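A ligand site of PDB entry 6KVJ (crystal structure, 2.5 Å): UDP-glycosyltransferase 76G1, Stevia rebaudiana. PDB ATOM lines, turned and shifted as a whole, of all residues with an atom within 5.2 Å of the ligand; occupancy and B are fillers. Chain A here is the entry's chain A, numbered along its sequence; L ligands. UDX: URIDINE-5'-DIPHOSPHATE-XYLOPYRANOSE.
Gln 24 touches the ligand. Gly 25 touches the ligand. CB of Ser 148 touches O4' of the ligand (3.9 Å). OH of Tyr 279 touches O4 of the ligand, 3.7 Å away. Ser 281 touches the ligand (OG to C5, 3.6 Å). Gly 283 touches the ligand. Val 310 touches the ligand (CG1 to O4, 3.6 Å). Trp 339 touches the ligand (CZ2 to C2, 3.2 Å). Gly 359 touches the ligand (C to O2A, 3.5 Å). Hydrophobic or aromatic side chains within 4 Å of the ligand: His 26, Val 310, Trp 339, Val 340, His 357 and Trp 360. 21 residues have an atom within 4 Å of the ligand: Gln 24, Gly 25, His 26, Asn 28, Thr 147, Ser 148, Tyr 279, Ser 281, Gly 283, Ser 284, Val 310, Trp 339, Val 340, Gln 342, His 357, Gly 359, Trp 360, Asn 361, Ser 362, Glu 365 and Asp 381. The nearest printed residue that does not touch the ligand is Thr 285 (4.04 Å).
An oxygen (O3') of the ligand lies within hydrogen-bond range of the side-chain hydroxyl (OG1) of Thr 147, at 3.3 Å. A ring nitrogen (NE2) of His 357 lies within hydrogen-bond range of an oxygen (O2B) of the ligand (2.8 Å). The backbone carbonyl oxygen (O) of Val 340 is in hydrogen-bond range of a nitrogen (N3) of the ligand (2.6 Å). An oxygen (O2D) of the ligand is in hydrogen-bond range of the side-chain carboxylate of Glu 365, at 2.7 Å. An oxygen (O1B) of the ligand is in hydrogen-bond range of the backbone NH of Ser 284 (3.0 Å). OG of Ser 362 lies within hydrogen-bond range of O1A of the ligand (2.6 Å). OD2 of Asp 381 is in hydrogen-bond range of O4' of the ligand (3.4 Å). An oxygen (O2A) of the ligand is in hydrogen-bond range of the backbone NH of Asn 361, at 3.1 Å. An oxygen (O1B) of the ligand is in hydrogen-bond range of the side-chain hydroxyl (OG) of Ser 284, at 2.5 Å. O4 of the ligand lies within hydrogen-bond range of N of Val 340 (3.2 Å). ND2 of Asn 361 is in hydrogen-bond range of O2A of the ligand (2.8 Å). A ring nitrogen (NE2) of His 26 sits at hydrogen-bond distance from an oxygen (O3') of the ligand, at 3.4 Å. An oxygen (O2A) of the ligand lies close to the backbone NH of Trp 360 (3.4 Å). ND2 of Asn 28 is in hydrogen-bond range of O3D of the ligand (3.1 Å). The backbone NH of Ser 362 is in hydrogen-bond range of an oxygen (O1A) of the ligand, 3.1 Å away. The side-chain amide nitrogen of Gln 342 lies close to an oxygen (O2D) of the ligand (3.3 Å).
The side-chain carboxylate (OE1) of Glu 365 sits at hydrogen-bond distance from the side-chain amide nitrogen (NE2) of Gln 342 (2.7 Å). The side-chain amide nitrogen (NE2) of Gln 342 lies within hydrogen-bond range of the side-chain hydroxyl (OG) of Ser 362, at 2.7 Å. The side-chain amide nitrogen (ND2) of Asn 361 sits at hydrogen-bond distance from the backbone carbonyl oxygen (O) of Gly 25 (3.0 Å). OE1 of Gln 382 lies close to O of His 357 (3.3 Å). The side-chain amide oxygen of Gln 342 lies within hydrogen-bond range of the side-chain hydroxyl of Tyr 279 (2.9 Å). The indole nitrogen (NE1) of Trp 339 sits at hydrogen-bond distance from the side-chain hydroxyl (OG) of Ser 257 (2.7 Å). The side-chain amide oxygen of Asn 28 is in hydrogen-bond range of the side-chain amide nitrogen of Gln 24, at 2.8 Å. A ring nitrogen (ND1) of His 357 sits close to the backbone NH (N) of Gly 359, 3.4 Å away.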
ATOM      1  N   GLN A  24      -5.946  18.105 -21.302  1.00  0.00           N
ATOM      2  CA  GLN A  24      -5.775  18.865 -22.550  1.00  0.00           C
ATOM      3  C   GLN A  24      -4.322  18.923 -22.996  1.00  0.00           C
ATOM      4  O   GLN A  24      -4.010  18.652 -24.161  1.00  0.00           O
ATOM      5  CB  GLN A  24      -6.343  20.276 -22.388  1.00  0.00           C
ATOM      6  CG  GLN A  24      -6.414  21.030 -23.707  1.00  0.00           C
ATOM      7  CD  GLN A  24      -7.533  20.531 -24.594  1.00  0.00           C
ATOM      8  OE1 GLN A  24      -8.709  20.930 -24.417  1.00  0.00           O
ATOM      9  NE2 GLN A  24      -7.197  19.632 -25.542  1.00  0.00           N
ATOM     10  N   GLY A  25      -3.419  19.258 -22.081  1.00  0.00           N
ATOM     11  CA  GLY A  25      -1.998  19.330 -22.387  1.00  0.00           C
ATOM     12  C   GLY A  25      -1.309  17.995 -22.596  1.00  0.00           C
ATOM     13  O   GLY A  25      -0.085  17.962 -22.814  1.00  0.00           O
ATOM     14  N   HIS A  26      -2.058  16.899 -22.529  1.00  0.00           N
ATOM     15  CA  HIS A  26      -1.511  15.587 -22.845  1.00  0.00           C
ATOM     16  C   HIS A  26      -2.075  14.971 -24.124  1.00  0.00           C
ATOM     17  O   HIS A  26      -1.296  14.402 -24.914  1.00  0.00           O
ATOM     18  CB  HIS A  26      -1.713  14.646 -21.668  1.00  0.00           C
ATOM     19  CG  HIS A  26      -0.932  15.042 -20.477  1.00  0.00           C
ATOM     20  ND1 HIS A  26       0.278  14.475 -20.153  1.00  0.00           N
ATOM     21  CD2 HIS A  26      -1.163  15.984 -19.537  1.00  0.00           C
ATOM     22  CE1 HIS A  26       0.739  15.031 -19.050  1.00  0.00           C
ATOM     23  NE2 HIS A  26      -0.117  15.950 -18.653  1.00  0.00           N
ATOM     24  N   ASN A  28      -3.438  16.763 -26.559  1.00  0.00           N
ATOM     25  CA  ASN A  28      -2.949  17.663 -27.617  1.00  0.00           C
ATOM     26  C   ASN A  28      -1.637  17.183 -28.194  1.00  0.00           C
ATOM     27  O   ASN A  28      -1.619  16.776 -29.380  1.00  0.00           O
ATOM     28  CB  ASN A  28      -2.878  19.098 -27.090  1.00  0.00           C
ATOM     29  CG  ASN A  28      -4.215  19.806 -27.149  1.00  0.00           C
ATOM     30  OD1 ASN A  28      -5.233  19.203 -27.485  1.00  0.00           O
ATOM     31  ND2 ASN A  28      -4.211  21.110 -26.847  1.00  0.00           N
ATOM     32  N   THR A 147       5.780  15.056 -22.515  1.00  0.00           N
ATOM     33  CA  THR A 147       4.966  16.247 -22.702  1.00  0.00           C
ATOM     34  C   THR A 147       5.562  17.519 -22.090  1.00  0.00           C
ATOM     35  O   THR A 147       5.020  18.597 -22.300  1.00  0.00           O
ATOM     36  CB  THR A 147       3.585  15.983 -22.110  1.00  0.00           C
ATOM     37  OG1 THR A 147       3.725  15.481 -20.768  1.00  0.00           O
ATOM     38  CG2 THR A 147       2.852  14.966 -22.966  1.00  0.00           C
ATOM     39  N   SER A 148       6.656  17.410 -21.340  1.00  0.00           N
ATOM     40  CA  SER A 148       7.388  18.581 -20.867  1.00  0.00           C
ATOM     41  C   SER A 148       8.802  18.539 -21.455  1.00  0.00           C
ATOM     42  O   SER A 148       9.139  17.672 -22.263  1.00  0.00           O
ATOM     43  CB  SER A 148       7.367  18.656 -19.335  1.00  0.00           C
ATOM     44  OG  SER A 148       7.427  17.352 -18.762  1.00  0.00           O
ATOM     45  N   ALA A 253      -3.166  21.829 -32.315  1.00  0.00           N
ATOM     46  CA  ALA A 253      -3.956  20.899 -31.519  1.00  0.00           C
ATOM     47  C   ALA A 253      -5.432  21.257 -31.540  1.00  0.00           C
ATOM     48  O   ALA A 253      -6.194  20.782 -30.669  1.00  0.00           O
ATOM     49  CB  ALA A 253      -3.435  20.862 -30.088  1.00  0.00           C
ATOM     50  N   SER A 257      -9.334  19.910 -29.054  1.00  0.00           N
ATOM     51  CA  SER A 257      -9.900  20.693 -27.968  1.00  0.00           C
ATOM     52  C   SER A 257     -10.997  19.905 -27.239  1.00  0.00           C
ATOM     53  O   SER A 257     -11.701  19.078 -27.839  1.00  0.00           O
ATOM     54  CB  SER A 257     -10.479  22.005 -28.523  1.00  0.00           C
ATOM     55  OG  SER A 257     -10.861  22.917 -27.505  1.00  0.00           O
ATOM     56  N   HIS A 261     -14.643  26.223 -29.249  1.00  0.00           N
ATOM     57  CA  HIS A 261     -13.910  27.445 -29.557  1.00  0.00           C
ATOM     58  C   HIS A 261     -14.873  28.637 -29.672  1.00  0.00           C
ATOM     59  O   HIS A 261     -16.002  28.502 -30.174  1.00  0.00           O
ATOM     60  CB  HIS A 261     -13.133  27.275 -30.857  1.00  0.00           C
ATOM     61  CG  HIS A 261     -12.130  26.167 -30.836  1.00  0.00           C
ATOM     62  ND1 HIS A 261     -11.221  26.012 -29.812  1.00  0.00           N
ATOM     63  CD2 HIS A 261     -11.891  25.165 -31.707  1.00  0.00           C
ATOM     64  CE1 HIS A 261     -10.462  24.959 -30.066  1.00  0.00           C
ATOM     65  NE2 HIS A 261     -10.857  24.424 -31.207  1.00  0.00           N
ATOM     66  N   TYR A 279      -2.142  38.581 -25.766  1.00  0.00           N
ATOM     67  CA  TYR A 279      -2.940  37.388 -25.489  1.00  0.00           C
ATOM     68  C   TYR A 279      -2.637  36.909 -24.062  1.00  0.00           C
ATOM     69  O   TYR A 279      -1.463  36.809 -23.682  1.00  0.00           O
ATOM     70  CB  TYR A 279      -2.651  36.297 -26.524  1.00  0.00           C
ATOM     71  CG  TYR A 279      -3.359  34.969 -26.299  1.00  0.00           C
ATOM     72  CD1 TYR A 279      -4.766  34.859 -26.362  1.00  0.00           C
ATOM     73  CD2 TYR A 279      -2.624  33.812 -26.058  1.00  0.00           C
ATOM     74  CE1 TYR A 279      -5.400  33.623 -26.166  1.00  0.00           C
ATOM     75  CE2 TYR A 279      -3.246  32.576 -25.854  1.00  0.00           C
ATOM     76  CZ  TYR A 279      -4.627  32.487 -25.905  1.00  0.00           C
ATOM     77  OH  TYR A 279      -5.227  31.261 -25.697  1.00  0.00           O
ATOM     78  N   SER A 281      -3.640  33.827 -21.205  1.00  0.00           N
ATOM     79  CA  SER A 281      -4.240  32.516 -20.954  1.00  0.00           C
ATOM     80  C   SER A 281      -3.375  31.751 -19.959  1.00  0.00           C
ATOM     81  O   SER A 281      -2.169  31.610 -20.158  1.00  0.00           O
ATOM     82  CB  SER A 281      -4.394  31.737 -22.257  1.00  0.00           C
ATOM     83  OG  SER A 281      -4.941  30.443 -22.009  1.00  0.00           O
ATOM     84  N   GLY A 283      -3.687  28.515 -18.984  1.00  0.00           N
ATOM     85  CA  GLY A 283      -3.736  27.074 -19.143  1.00  0.00           C
ATOM     86  C   GLY A 283      -5.138  26.500 -19.060  1.00  0.00           C
ATOM     87  O   GLY A 283      -6.162  27.187 -19.183  1.00  0.00           O
ATOM     88  N   SER A 284      -5.177  25.190 -18.826  1.00  0.00           N
ATOM     89  CA  SER A 284      -6.436  24.468 -18.722  1.00  0.00           C
ATOM     90  C   SER A 284      -6.772  23.987 -17.313  1.00  0.00           C
ATOM     91  O   SER A 284      -7.859  23.442 -17.105  1.00  0.00           O
ATOM     92  CB  SER A 284      -6.437  23.257 -19.668  1.00  0.00           C
ATOM     93  OG  SER A 284      -5.546  22.241 -19.232  1.00  0.00           O
ATOM     94  N   THR A 285      -5.892  24.199 -16.355  1.00  0.00           N
ATOM     95  CA  THR A 285      -6.083  23.623 -15.046  1.00  0.00           C
ATOM     96  C   THR A 285      -5.946  24.627 -13.936  1.00  0.00           C
ATOM     97  O   THR A 285      -6.354  24.366 -12.840  1.00  0.00           O
ATOM     98  CB  THR A 285      -5.187  22.387 -14.787  1.00  0.00           C
ATOM     99  OG1 THR A 285      -4.006  22.771 -14.094  1.00  0.00           O
ATOM    100  CG2 THR A 285      -4.775  21.760 -16.047  1.00  0.00           C
ATOM    101  N   VAL A 310      -8.277  34.791 -22.199  1.00  0.00           N
ATOM    102  CA  VAL A 310      -9.066  33.580 -21.972  1.00  0.00           C
ATOM    103  C   VAL A 310      -9.135  33.330 -20.467  1.00  0.00           C
ATOM    104  O   VAL A 310      -8.111  33.120 -19.811  1.00  0.00           O
ATOM    105  CB  VAL A 310      -8.461  32.372 -22.708  1.00  0.00           C
ATOM    106  CG1 VAL A 310      -9.215  31.091 -22.325  1.00  0.00           C
ATOM    107  CG2 VAL A 310      -8.472  32.573 -24.231  1.00  0.00           C
ATOM    108  N   TRP A 339     -12.596  30.314 -24.078  1.00  0.00           N
ATOM    109  CA  TRP A 339     -11.751  29.314 -24.740  1.00  0.00           C
ATOM    110  C   TRP A 339     -11.573  29.673 -26.212  1.00  0.00           C
ATOM    111  O   TRP A 339     -12.547  30.019 -26.887  1.00  0.00           O
ATOM    112  CB  TRP A 339     -12.372  27.925 -24.608  1.00  0.00           C
ATOM    113  CG  TRP A 339     -11.414  26.821 -24.918  1.00  0.00           C
ATOM    114  CD1 TRP A 339     -11.389  26.047 -26.043  1.00  0.00           C
ATOM    115  CD2 TRP A 339     -10.328  26.360 -24.086  1.00  0.00           C
ATOM    116  NE1 TRP A 339     -10.357  25.128 -25.972  1.00  0.00           N
ATOM    117  CE2 TRP A 339      -9.691  25.298 -24.786  1.00  0.00           C
ATOM    118  CE3 TRP A 339      -9.832  26.744 -22.832  1.00  0.00           C
ATOM    119  CZ2 TRP A 339      -8.577  24.614 -24.270  1.00  0.00           C
ATOM    120  CZ3 TRP A 339      -8.718  26.061 -22.315  1.00  0.00           C
ATOM    121  CH2 TRP A 339      -8.107  25.006 -23.043  1.00  0.00           C
ATOM    122  N   VAL A 340     -10.344  29.565 -26.720  1.00  0.00           N
ATOM    123  CA  VAL A 340     -10.039  29.897 -28.113  1.00  0.00           C
ATOM    124  C   VAL A 340      -9.241  28.773 -28.747  1.00  0.00           C
ATOM    125  O   VAL A 340      -8.658  27.931 -28.042  1.00  0.00           O
ATOM    126  CB  VAL A 340      -9.257  31.237 -28.232  1.00  0.00           C
ATOM    127  CG1 VAL A 340      -9.985  32.360 -27.509  1.00  0.00           C
ATOM    128  CG2 VAL A 340      -7.835  31.072 -27.710  1.00  0.00           C
ATOM    129  N   PRO A 341      -9.144  28.735 -30.074  1.00  0.00           N
ATOM    130  CA  PRO A 341      -8.086  27.912 -30.682  1.00  0.00           C
ATOM    131  C   PRO A 341      -6.744  28.610 -30.512  1.00  0.00           C
ATOM    132  O   PRO A 341      -6.357  29.452 -31.333  1.00  0.00           O
ATOM    133  CB  PRO A 341      -8.509  27.774 -32.151  1.00  0.00           C
ATOM    134  CG  PRO A 341      -9.591  28.833 -32.387  1.00  0.00           C
ATOM    135  CD  PRO A 341      -9.862  29.550 -31.076  1.00  0.00           C
ATOM    136  N   GLN A 342      -6.022  28.240 -29.449  1.00  0.00           N
ATOM    137  CA  GLN A 342      -4.941  29.073 -28.911  1.00  0.00           C
ATOM    138  C   GLN A 342      -3.845  29.327 -29.947  1.00  0.00           C
ATOM    139  O   GLN A 342      -3.397  30.479 -30.112  1.00  0.00           O
ATOM    140  CB  GLN A 342      -4.341  28.426 -27.658  1.00  0.00           C
ATOM    141  CG  GLN A 342      -3.033  29.068 -27.277  1.00  0.00           C
ATOM    142  CD  GLN A 342      -2.638  28.796 -25.847  1.00  0.00           C
ATOM    143  OE1 GLN A 342      -3.259  29.306 -24.907  1.00  0.00           O
ATOM    144  NE2 GLN A 342      -1.597  27.972 -25.677  1.00  0.00           N
ATOM    145  N   GLN A 343      -3.379  28.287 -30.644  1.00  0.00           N
ATOM    146  CA  GLN A 343      -2.233  28.493 -31.509  1.00  0.00           C
ATOM    147  C   GLN A 343      -2.604  29.322 -32.733  1.00  0.00           C
ATOM    148  O   GLN A 343      -1.784  30.116 -33.217  1.00  0.00           O
ATOM    149  CB  GLN A 343      -1.586  27.159 -31.926  1.00  0.00           C
ATOM    150  CG  GLN A 343      -0.517  27.328 -33.006  1.00  0.00           C
ATOM    151  CD  GLN A 343       0.400  26.110 -33.209  1.00  0.00           C
ATOM    152  OE1 GLN A 343       1.468  26.240 -33.819  1.00  0.00           O
ATOM    153  NE2 GLN A 343      -0.009  24.930 -32.687  1.00  0.00           N
ATOM    154  N   HIS A 357       0.967  30.970 -18.431  1.00  0.00           N
ATOM    155  CA  HIS A 357       1.295  30.289 -17.188  1.00  0.00           C
ATOM    156  C   HIS A 357       2.474  29.336 -17.340  1.00  0.00           C
ATOM    157  O   HIS A 357       2.745  28.546 -16.430  1.00  0.00           O
ATOM    158  CB  HIS A 357       0.079  29.529 -16.654  1.00  0.00           C
ATOM    159  CG  HIS A 357      -0.175  28.223 -17.336  1.00  0.00           C
ATOM    160  ND1 HIS A 357      -0.158  28.082 -18.703  1.00  0.00           N
ATOM    161  CD2 HIS A 357      -0.450  26.990 -16.835  1.00  0.00           C
ATOM    162  CE1 HIS A 357      -0.405  26.823 -19.020  1.00  0.00           C
ATOM    163  NE2 HIS A 357      -0.575  26.134 -17.906  1.00  0.00           N
ATOM    164  N   GLY A 359       2.918  26.674 -19.086  1.00  0.00           N
ATOM    165  CA  GLY A 359       2.709  25.295 -19.509  1.00  0.00           C
ATOM    166  C   GLY A 359       3.503  24.998 -20.764  1.00  0.00           C
ATOM    167  O   GLY A 359       3.640  25.845 -21.655  1.00  0.00           O
ATOM    168  N   TRP A 360       4.043  23.764 -20.841  1.00  0.00           N
ATOM    169  CA  TRP A 360       5.038  23.516 -21.888  1.00  0.00           C
ATOM    170  C   TRP A 360       4.422  23.555 -23.279  1.00  0.00           C
ATOM    171  O   TRP A 360       5.081  23.983 -24.235  1.00  0.00           O
ATOM    172  CB  TRP A 360       5.784  22.193 -21.668  1.00  0.00           C
ATOM    173  CG  TRP A 360       6.883  22.016 -22.737  1.00  0.00           C
ATOM    174  CD1 TRP A 360       6.891  21.123 -23.790  1.00  0.00           C
ATOM    175  CD2 TRP A 360       8.057  22.827 -22.897  1.00  0.00           C
ATOM    176  NE1 TRP A 360       8.026  21.297 -24.545  1.00  0.00           N
ATOM    177  CE2 TRP A 360       8.754  22.342 -24.032  1.00  0.00           C
ATOM    178  CE3 TRP A 360       8.593  23.906 -22.183  1.00  0.00           C
ATOM    179  CZ2 TRP A 360       9.940  22.887 -24.458  1.00  0.00           C
ATOM    180  CZ3 TRP A 360       9.781  24.452 -22.598  1.00  0.00           C
ATOM    181  CH2 TRP A 360      10.443  23.938 -23.743  1.00  0.00           C
ATOM    182  N   ASN A 361       3.162  23.138 -23.434  1.00  0.00           N
ATOM    183  CA  ASN A 361       2.557  23.238 -24.753  1.00  0.00           C
ATOM    184  C   ASN A 361       2.378  24.686 -25.165  1.00  0.00           C
ATOM    185  O   ASN A 361       2.735  25.079 -26.278  1.00  0.00           O
ATOM    186  CB  ASN A 361       1.215  22.535 -24.819  1.00  0.00           C
ATOM    187  CG  ASN A 361       1.323  21.080 -24.546  1.00  0.00           C
ATOM    188  OD1 ASN A 361       1.584  20.282 -25.461  1.00  0.00           O
ATOM    189  ND2 ASN A 361       1.038  20.685 -23.283  1.00  0.00           N
ATOM    190  N   SER A 362       1.783  25.499 -24.294  1.00  0.00           N
ATOM    191  CA  SER A 362       1.586  26.901 -24.623  1.00  0.00           C
ATOM    192  C   SER A 362       2.924  27.561 -24.963  1.00  0.00           C
ATOM    193  O   SER A 362       3.058  28.235 -25.995  1.00  0.00           O
ATOM    194  CB  SER A 362       0.883  27.621 -23.478  1.00  0.00           C
ATOM    195  OG  SER A 362      -0.465  27.185 -23.395  1.00  0.00           O
ATOM    196  N   GLU A 365       4.145  26.461 -28.283  1.00  0.00           N
ATOM    197  CA  GLU A 365       3.281  27.062 -29.296  1.00  0.00           C
ATOM    198  C   GLU A 365       3.704  28.502 -29.569  1.00  0.00           C
ATOM    199  O   GLU A 365       3.889  28.909 -30.729  1.00  0.00           O
ATOM    200  CB  GLU A 365       1.817  26.984 -28.846  1.00  0.00           C
ATOM    201  CG  GLU A 365       1.184  25.560 -29.016  1.00  0.00           C
ATOM    202  CD  GLU A 365      -0.107  25.317 -28.187  1.00  0.00           C
ATOM    203  OE1 GLU A 365      -0.659  26.279 -27.573  1.00  0.00           O
ATOM    204  OE2 GLU A 365      -0.563  24.146 -28.152  1.00  0.00           O
ATOM    205  N   ASP A 381       6.413  22.035 -13.552  1.00  0.00           N
ATOM    206  CA  ASP A 381       7.462  22.328 -14.490  1.00  0.00           C
ATOM    207  C   ASP A 381       7.473  23.764 -14.973  1.00  0.00           C
ATOM    208  O   ASP A 381       8.411  24.190 -15.555  1.00  0.00           O
ATOM    209  CB  ASP A 381       7.416  21.367 -15.678  1.00  0.00           C
ATOM    210  CG  ASP A 381       6.208  21.551 -16.517  1.00  0.00           C
ATOM    211  OD1 ASP A 381       5.110  21.565 -15.972  1.00  0.00           O
ATOM    212  OD2 ASP A 381       6.354  21.668 -17.731  1.00  0.00           O
ATOM    213  N   GLN A 382       6.414  24.487 -14.680  1.00  0.00           N
ATOM    214  CA  GLN A 382       6.194  25.846 -15.102  1.00  0.00           C
ATOM    215  C   GLN A 382       7.223  26.880 -14.664  1.00  0.00           C
ATOM    216  O   GLN A 382       7.654  27.638 -15.482  1.00  0.00           O
ATOM    217  CB  GLN A 382       4.771  26.251 -14.729  1.00  0.00           C
ATOM    218  CG  GLN A 382       3.747  25.331 -15.349  1.00  0.00           C
ATOM    219  CD  GLN A 382       2.371  25.452 -14.760  1.00  0.00           C
ATOM    220  OE1 GLN A 382       2.097  26.336 -14.009  1.00  0.00           O
ATOM    221  NE2 GLN A 382       1.529  24.533 -15.090  1.00  0.00           N
HETATM  222  C1' UDX L   1      -0.076  21.154 -19.278  1.00  0.00           C
HETATM  223  C2' UDX L   1       0.210  19.679 -19.184  1.00  0.00           C
HETATM  224  O2' UDX L   1      -0.250  19.321 -17.889  1.00  0.00           O
HETATM  225  C3' UDX L   1       1.694  19.357 -19.191  1.00  0.00           C
HETATM  226  O3' UDX L   1       2.031  18.249 -19.986  1.00  0.00           O
HETATM  227  C4' UDX L   1       2.497  20.516 -19.681  1.00  0.00           C
HETATM  228  O4' UDX L   1       3.801  20.186 -19.358  1.00  0.00           O
HETATM  229  C5' UDX L   1       2.170  21.732 -18.841  1.00  0.00           C
HETATM  230  O5' UDX L   1       0.826  21.755 -18.349  1.00  0.00           O
HETATM  231  PB  UDX L   1      -1.904  22.947 -19.146  1.00  0.00           P
HETATM  232  O1B UDX L   1      -3.246  23.059 -19.656  1.00  0.00           O
HETATM  233  O2B UDX L   1      -1.682  23.582 -17.899  1.00  0.00           O
HETATM  234  O3B UDX L   1      -1.428  21.491 -18.982  1.00  0.00           O
HETATM  235  O3A UDX L   1      -0.832  23.658 -20.065  1.00  0.00           O
HETATM  236  PA  UDX L   1      -0.354  23.640 -21.549  1.00  0.00           P
HETATM  237  O1A UDX L   1      -0.251  25.002 -21.948  1.00  0.00           O
HETATM  238  O2A UDX L   1       0.814  22.819 -21.510  1.00  0.00           O
HETATM  239  O5D UDX L   1      -1.401  22.991 -22.461  1.00  0.00           O
HETATM  240  C5D UDX L   1      -2.591  23.662 -22.691  1.00  0.00           C
HETATM  241  C4D UDX L   1      -3.145  23.465 -24.072  1.00  0.00           C
HETATM  242  O4D UDX L   1      -4.379  24.130 -24.106  1.00  0.00           O
HETATM  243  C3D UDX L   1      -2.311  24.129 -25.130  1.00  0.00           C
HETATM  244  O3D UDX L   1      -1.964  23.157 -26.090  1.00  0.00           O
HETATM  245  C2D UDX L   1      -3.194  25.213 -25.711  1.00  0.00           C
HETATM  246  O2D UDX L   1      -3.114  25.367 -27.112  1.00  0.00           O
HETATM  247  C1D UDX L   1      -4.557  24.743 -25.330  1.00  0.00           C
HETATM  248  N1  UDX L   1      -5.429  25.861 -25.165  1.00  0.00           N
HETATM  249  C6  UDX L   1      -5.318  26.651 -24.133  1.00  0.00           C
HETATM  250  C2  UDX L   1      -6.416  26.114 -26.113  1.00  0.00           C
HETATM  251  O2  UDX L   1      -6.550  25.384 -27.086  1.00  0.00           O
HETATM  252  N3  UDX L   1      -7.231  27.114 -25.964  1.00  0.00           N
HETATM  253  C4  UDX L   1      -7.129  27.925 -24.933  1.00  0.00           C
HETATM  254  O4  UDX L   1      -7.882  28.857 -24.798  1.00  0.00           O
HETATM  255  C5  UDX L   1      -6.168  27.724 -23.986  1.00  0.00           C
